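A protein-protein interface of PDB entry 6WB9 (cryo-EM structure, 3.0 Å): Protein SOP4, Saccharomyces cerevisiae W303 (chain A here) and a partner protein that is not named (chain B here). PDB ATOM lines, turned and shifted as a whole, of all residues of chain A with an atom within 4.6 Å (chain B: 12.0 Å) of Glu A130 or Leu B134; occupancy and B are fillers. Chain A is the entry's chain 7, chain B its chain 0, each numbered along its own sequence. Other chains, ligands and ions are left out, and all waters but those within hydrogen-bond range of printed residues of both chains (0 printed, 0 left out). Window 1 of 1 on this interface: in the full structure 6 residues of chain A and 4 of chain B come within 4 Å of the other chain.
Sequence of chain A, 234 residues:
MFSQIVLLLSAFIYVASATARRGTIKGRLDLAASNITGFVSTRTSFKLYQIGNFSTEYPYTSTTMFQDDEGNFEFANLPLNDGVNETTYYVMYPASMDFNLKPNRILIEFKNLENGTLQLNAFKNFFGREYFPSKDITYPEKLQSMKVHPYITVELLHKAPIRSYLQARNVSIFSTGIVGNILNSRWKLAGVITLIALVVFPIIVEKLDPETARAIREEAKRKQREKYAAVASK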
ATOM      1  N   ASN A 125       9.618 -13.054  14.688  1.00  0.00           N
ATOM      2  CA  ASN A 125       9.010 -13.095  16.008  1.00  0.00           C
ATOM      3  C   ASN A 125       7.849 -12.116  16.021  1.00  0.00           C
ATOM      4  O   ASN A 125       7.871 -11.102  15.324  1.00  0.00           O
ATOM      5  CB  ASN A 125      10.019 -12.746  17.105  1.00  0.00           C
ATOM      6  CG  ASN A 125       9.533 -13.123  18.481  1.00  0.00           C
ATOM      7  OD1 ASN A 125       8.520 -13.802  18.626  1.00  0.00           O
ATOM      8  ND2 ASN A 125      10.255 -12.692  19.503  1.00  0.00           N
ATOM      9  N   GLY A 128       5.219  -9.672  21.907  1.00  0.00           N
ATOM     10  CA  GLY A 128       4.759 -10.309  23.113  1.00  0.00           C
ATOM     11  C   GLY A 128       5.319 -11.685  23.374  1.00  0.00           C
ATOM     12  O   GLY A 128       4.722 -12.435  24.150  1.00  0.00           O
ATOM     13  N   ARG A 129       6.442 -12.040  22.756  1.00  0.00           N
ATOM     14  CA  ARG A 129       7.077 -13.331  22.958  1.00  0.00           C
ATOM     15  C   ARG A 129       8.571 -13.108  23.122  1.00  0.00           C
ATOM     16  O   ARG A 129       9.138 -12.212  22.494  1.00  0.00           O
ATOM     17  CB  ARG A 129       6.792 -14.286  21.786  1.00  0.00           C
ATOM     18  CG  ARG A 129       7.283 -15.716  21.984  1.00  0.00           C
ATOM     19  CD  ARG A 129       6.741 -16.650  20.925  1.00  0.00           C
ATOM     20  NE  ARG A 129       7.199 -16.292  19.588  1.00  0.00           N
ATOM     21  CZ  ARG A 129       7.882 -17.104  18.789  1.00  0.00           C
ATOM     22  NH1 ARG A 129       8.180 -18.332  19.188  1.00  0.00           N
ATOM     23  NH2 ARG A 129       8.255 -16.693  17.587  1.00  0.00           N
ATOM     24  N   GLU A 130       9.198 -13.913  23.978  1.00  0.00           N
ATOM     25  CA  GLU A 130      10.626 -13.809  24.227  1.00  0.00           C
ATOM     26  C   GLU A 130      11.422 -14.218  22.990  1.00  0.00           C
ATOM     27  O   GLU A 130      10.918 -14.879  22.080  1.00  0.00           O
ATOM     28  CB  GLU A 130      11.024 -14.677  25.419  1.00  0.00           C
ATOM     29  CG  GLU A 130      12.134 -14.094  26.276  1.00  0.00           C
ATOM     30  CD  GLU A 130      12.711 -15.103  27.248  1.00  0.00           C
ATOM     31  OE1 GLU A 130      12.221 -16.253  27.276  1.00  0.00           O
ATOM     32  OE2 GLU A 130      13.659 -14.747  27.980  1.00  0.00           O
ATOM     33  N   TYR A 131      12.688 -13.806  22.963  1.00  0.00           N
ATOM     34  CA  TYR A 131      13.542 -14.012  21.803  1.00  0.00           C
ATOM     35  C   TYR A 131      14.521 -15.158  21.981  1.00  0.00           C
ATOM     36  O   TYR A 131      14.994 -15.712  20.984  1.00  0.00           O
ATOM     37  CB  TYR A 131      14.319 -12.728  21.476  1.00  0.00           C
ATOM     38  CG  TYR A 131      13.443 -11.603  20.978  1.00  0.00           C
ATOM     39  CD1 TYR A 131      13.323 -11.332  19.621  1.00  0.00           C
ATOM     40  CD2 TYR A 131      12.727 -10.816  21.867  1.00  0.00           C
ATOM     41  CE1 TYR A 131      12.515 -10.309  19.172  1.00  0.00           C
ATOM     42  CE2 TYR A 131      11.914  -9.815  21.427  1.00  0.00           C
ATOM     43  CZ  TYR A 131      11.815  -9.557  20.092  1.00  0.00           C
ATOM     44  OH  TYR A 131      11.000  -8.532  19.702  1.00  0.00           O
ATOM     45  N   PHE A 132      14.838 -15.521  23.218  1.00  0.00           N
ATOM     46  CA  PHE A 132      15.683 -16.656  23.504  1.00  0.00           C
ATOM     47  C   PHE A 132      14.949 -17.620  24.426  1.00  0.00           C
ATOM     48  O   PHE A 132      14.231 -17.179  25.329  1.00  0.00           O
ATOM     49  CB  PHE A 132      16.992 -16.211  24.165  1.00  0.00           C
ATOM     50  CG  PHE A 132      17.602 -15.002  23.530  1.00  0.00           C
ATOM     51  CD1 PHE A 132      18.190 -15.085  22.282  1.00  0.00           C
ATOM     52  CD2 PHE A 132      17.591 -13.783  24.186  1.00  0.00           C
ATOM     53  CE1 PHE A 132      18.754 -13.973  21.696  1.00  0.00           C
ATOM     54  CE2 PHE A 132      18.156 -12.665  23.605  1.00  0.00           C
ATOM     55  CZ  PHE A 132      18.738 -12.762  22.359  1.00  0.00           C
ATOM     56  N   PRO A 133      15.092 -18.925  24.224  1.00  0.00           N
ATOM     57  CA  PRO A 133      14.430 -19.886  25.107  1.00  0.00           C
ATOM     58  C   PRO A 133      15.125 -19.946  26.460  1.00  0.00           C
ATOM     59  O   PRO A 133      16.245 -19.468  26.640  1.00  0.00           O
ATOM     60  CB  PRO A 133      14.566 -21.208  24.351  1.00  0.00           C
ATOM     61  CG  PRO A 133      15.816 -21.045  23.568  1.00  0.00           C
ATOM     62  CD  PRO A 133      15.868 -19.597  23.168  1.00  0.00           C
ATOM     63  N   ILE A 137      15.174 -25.779  29.181  1.00  0.00           N
ATOM     64  CA  ILE A 137      14.699 -26.585  28.065  1.00  0.00           C
ATOM     65  C   ILE A 137      15.831 -26.865  27.085  1.00  0.00           C
ATOM     66  O   ILE A 137      15.942 -27.966  26.545  1.00  0.00           O
ATOM     67  CB  ILE A 137      13.523 -25.899  27.353  1.00  0.00           C
ATOM     68  CG1 ILE A 137      12.625 -25.191  28.368  1.00  0.00           C
ATOM     69  CG2 ILE A 137      12.717 -26.916  26.566  1.00  0.00           C
ATOM     70  CD1 ILE A 137      11.498 -24.404  27.741  1.00  0.00           C
ATOM     71  N   GLN A 144      11.376 -24.729  21.598  1.00  0.00           N
ATOM     72  CA  GLN A 144      10.755 -24.225  20.383  1.00  0.00           C
ATOM     73  C   GLN A 144      11.627 -23.137  19.772  1.00  0.00           C
ATOM     74  O   GLN A 144      12.065 -22.219  20.468  1.00  0.00           O
ATOM     75  CB  GLN A 144       9.359 -23.684  20.683  1.00  0.00           C
ATOM     76  CG  GLN A 144       8.661 -23.068  19.486  1.00  0.00           C
ATOM     77  CD  GLN A 144       7.316 -22.471  19.842  1.00  0.00           C
ATOM     78  OE1 GLN A 144       6.758 -22.757  20.900  1.00  0.00           O
ATOM     79  NE2 GLN A 144       6.789 -21.634  18.959  1.00  0.00           N
ATOM     80  N   MET A 146      12.403 -20.121  16.720  1.00  0.00           N
ATOM     81  CA  MET A 146      11.718 -19.087  15.965  1.00  0.00           C
ATOM     82  C   MET A 146      11.927 -19.310  14.474  1.00  0.00           C
ATOM     83  O   MET A 146      12.947 -19.858  14.049  1.00  0.00           O
ATOM     84  CB  MET A 146      12.217 -17.700  16.369  1.00  0.00           C
ATOM     85  CG  MET A 146      11.646 -17.211  17.684  1.00  0.00           C
ATOM     86  SD  MET A 146      12.804 -16.199  18.610  1.00  0.00           S
ATOM     87  CE  MET A 146      13.094 -14.870  17.456  1.00  0.00           C
ATOM     88  N   THR B 128       7.240  -7.582  36.689  1.00  0.00           N
ATOM     89  CA  THR B 128       7.734  -8.009  35.395  1.00  0.00           C
ATOM     90  C   THR B 128       6.578  -8.647  34.644  1.00  0.00           C
ATOM     91  O   THR B 128       5.740  -9.324  35.247  1.00  0.00           O
ATOM     92  CB  THR B 128       8.893  -8.994  35.546  1.00  0.00           C
ATOM     93  OG1 THR B 128       9.726  -8.581  36.636  1.00  0.00           O
ATOM     94  CG2 THR B 128       9.729  -9.023  34.293  1.00  0.00           C
ATOM     95  N   ALA B 129       6.522  -8.415  33.338  1.00  0.00           N
ATOM     96  CA  ALA B 129       5.336  -8.980  32.714  1.00  0.00           C
ATOM     97  C   ALA B 129       5.598 -10.412  32.257  1.00  0.00           C
ATOM     98  O   ALA B 129       6.682 -10.714  31.752  1.00  0.00           O
ATOM     99  CB  ALA B 129       4.899  -8.141  31.524  1.00  0.00           C
ATOM    100  N   PRO B 130       4.630 -11.302  32.442  1.00  0.00           N
ATOM    101  CA  PRO B 130       4.763 -12.657  31.900  1.00  0.00           C
ATOM    102  C   PRO B 130       4.535 -12.706  30.396  1.00  0.00           C
ATOM    103  O   PRO B 130       3.425 -12.989  29.934  1.00  0.00           O
ATOM    104  CB  PRO B 130       3.692 -13.445  32.661  1.00  0.00           C
ATOM    105  CG  PRO B 130       2.711 -12.429  33.099  1.00  0.00           C
ATOM    106  CD  PRO B 130       3.487 -11.185  33.360  1.00  0.00           C
ATOM    107  N   VAL B 131       5.583 -12.419  29.621  1.00  0.00           N
ATOM    108  CA  VAL B 131       5.489 -12.556  28.174  1.00  0.00           C
ATOM    109  C   VAL B 131       5.477 -14.033  27.791  1.00  0.00           C
ATOM    110  O   VAL B 131       5.780 -14.921  28.595  1.00  0.00           O
ATOM    111  CB  VAL B 131       6.639 -11.813  27.479  1.00  0.00           C
ATOM    112  CG1 VAL B 131       6.615 -10.350  27.854  1.00  0.00           C
ATOM    113  CG2 VAL B 131       7.970 -12.440  27.847  1.00  0.00           C
ATOM    114  N   THR B 132       5.107 -14.292  26.538  1.00  0.00           N
ATOM    115  CA  THR B 132       5.053 -15.656  26.031  1.00  0.00           C
ATOM    116  C   THR B 132       6.458 -16.232  25.906  1.00  0.00           C
ATOM    117  O   THR B 132       7.373 -15.577  25.403  1.00  0.00           O
ATOM    118  CB  THR B 132       4.353 -15.691  24.675  1.00  0.00           C
ATOM    119  OG1 THR B 132       3.162 -14.898  24.733  1.00  0.00           O
ATOM    120  CG2 THR B 132       3.978 -17.108  24.300  1.00  0.00           C
ATOM    121  N   LYS B 133       6.630 -17.458  26.381  1.00  0.00           N
ATOM    122  CA  LYS B 133       7.923 -18.120  26.357  1.00  0.00           C
ATOM    123  C   LYS B 133       8.048 -19.005  25.125  1.00  0.00           C
ATOM    124  O   LYS B 133       7.084 -19.253  24.397  1.00  0.00           O
ATOM    125  CB  LYS B 133       8.137 -18.947  27.629  1.00  0.00           C
ATOM    126  CG  LYS B 133       8.744 -18.175  28.793  1.00  0.00           C
ATOM    127  CD  LYS B 133       7.690 -17.425  29.580  1.00  0.00           C
ATOM    128  CE  LYS B 133       8.316 -16.484  30.591  1.00  0.00           C
ATOM    129  NZ  LYS B 133       7.285 -15.669  31.292  1.00  0.00           N
ATOM    130  N   LEU B 134       9.266 -19.483  24.896  1.00  0.00           N
ATOM    131  CA  LEU B 134       9.564 -20.407  23.810  1.00  0.00           C
ATOM    132  C   LEU B 134       9.444 -21.822  24.360  1.00  0.00           C
ATOM    133  O   LEU B 134      10.317 -22.286  25.099  1.00  0.00           O
ATOM    134  CB  LEU B 134      10.956 -20.143  23.238  1.00  0.00           C
ATOM    135  CG  LEU B 134      11.036 -19.383  21.913  1.00  0.00           C
ATOM    136  CD1 LEU B 134      10.214 -18.120  21.951  1.00  0.00           C
ATOM    137  CD2 LEU B 134      12.477 -19.059  21.582  1.00  0.00           C
ATOM    138  N   LYS B 135       8.359 -22.499  24.001  1.00  0.00           N
ATOM    139  CA  LYS B 135       8.028 -23.796  24.574  1.00  0.00           C
ATOM    140  C   LYS B 135       8.916 -24.909  24.031  1.00  0.00           C
ATOM    141  O   LYS B 135       9.251 -25.854  24.748  1.00  0.00           O
ATOM    142  CB  LYS B 135       6.557 -24.117  24.309  1.00  0.00           C
ATOM    143  CG  LYS B 135       5.615 -23.013  24.751  1.00  0.00           C
ATOM    144  CD  LYS B 135       4.197 -23.258  24.270  1.00  0.00           C
ATOM    145  CE  LYS B 135       3.272 -22.132  24.708  1.00  0.00           C
ATOM    146  NZ  LYS B 135       1.860 -22.373  24.299  1.00  0.00           N
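Of the printed residues of chain B, Glu A130 touches Thr B132 and Leu B134. Of chain A, only Arg A129 (3.4 Å), Glu A130 (3.3 Å), Pro A133 (3.7 Å), Ile A137 (3.6 Å) and Gln A144 (3.3 Å) come within 4 Å of Leu B134. Of chain B, only Val B131 (3.9 Å) and Thr B132 (3.0 Å) come within 4 Å of Gly A128. No residue of chain B comes within 4 Å of Tyr A131. No residue of chain B comes within 4 Å of Phe A132. Pro A133 touches one residue of chain B. Of chain B, only Leu B134 and Lys B135 come within 4 Å of Gln A144. Met A146 touches none of the printed residues of chain B. Printed residues of chain A within 4 Å of Val B131: Gly A128 (3.9 Å). Printed residues of chain A within 4 Å of Lys B135: Gln A144. Of the printed residues of chain A, Thr B132 touches Gly A128 (3.0 Å), Arg A129 (3.3 Å) and Glu A130 (2.9 Å). Printed residues of chain B within 4 Å of Ile A137: Leu B134 (3.6 Å). The nearest residue of chain B that does not touch Glu A130 is Lys B133 (4.3 Å). The nearest residue of chain A that does not touch Leu B134 is Phe A132 (4.03 Å). The nearest printed residue of chain B that does not touch Ile A137 is Lys B135 (4.01 Å).
Printed residues of chain A that touch a printed residue of chain B: Gly A128, Arg A129, Glu A130, Pro A133, Ile A137 and Gln A144. Hydrophobic or aromatic side chains of chain A within 4 Å of the printed part of chain B: Pro A133 and Ile A137. Of the 8 printed residues of chain B, 4 touch a printed residue of chain A. Hydrophobic or aromatic side chains of chain B that line the printed part of chain A: Val B131 and Leu B134. Along chain B the printed residues that touch a printed residue of chain A span positions 131 to 135. Among the printed residues, 10 pairs touch across the chains.
The side-chain hydroxyl (OG1) of Thr B132 sits at hydrogen-bond distance from the backbone carbonyl oxygen (O) of Gly A128 (3.0 Å). N of Lys B135 sits at hydrogen-bond distance from OE1 of Gln A144, 3.5 Å away. The backbone carbonyl oxygen of Thr B132 is in hydrogen-bond range of the backbone NH of Glu A130 (2.9 Å).
Among the printed residues, pairs that only touch across the chains: Glu A130 with Leu B134, Arg A129 with Thr B132, Gln A144 with Leu B134, Arg A129 with Leu B134, Ile A137 with Leu B134, Pro A133 with Leu B134 and Gly A128 with Val B131.
NE of Arg A129 sits at hydrogen-bond distance from OD1 of Asn A125, 3.0 Å away. The side-chain amide nitrogen (ND2) of Asn A125 lies within hydrogen-bond range of the backbone carbonyl oxygen (O) of Glu A130 (3.4 Å). NZ of Lys B133 lies within hydrogen-bond range of O of Val B131 (3.2 Å).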
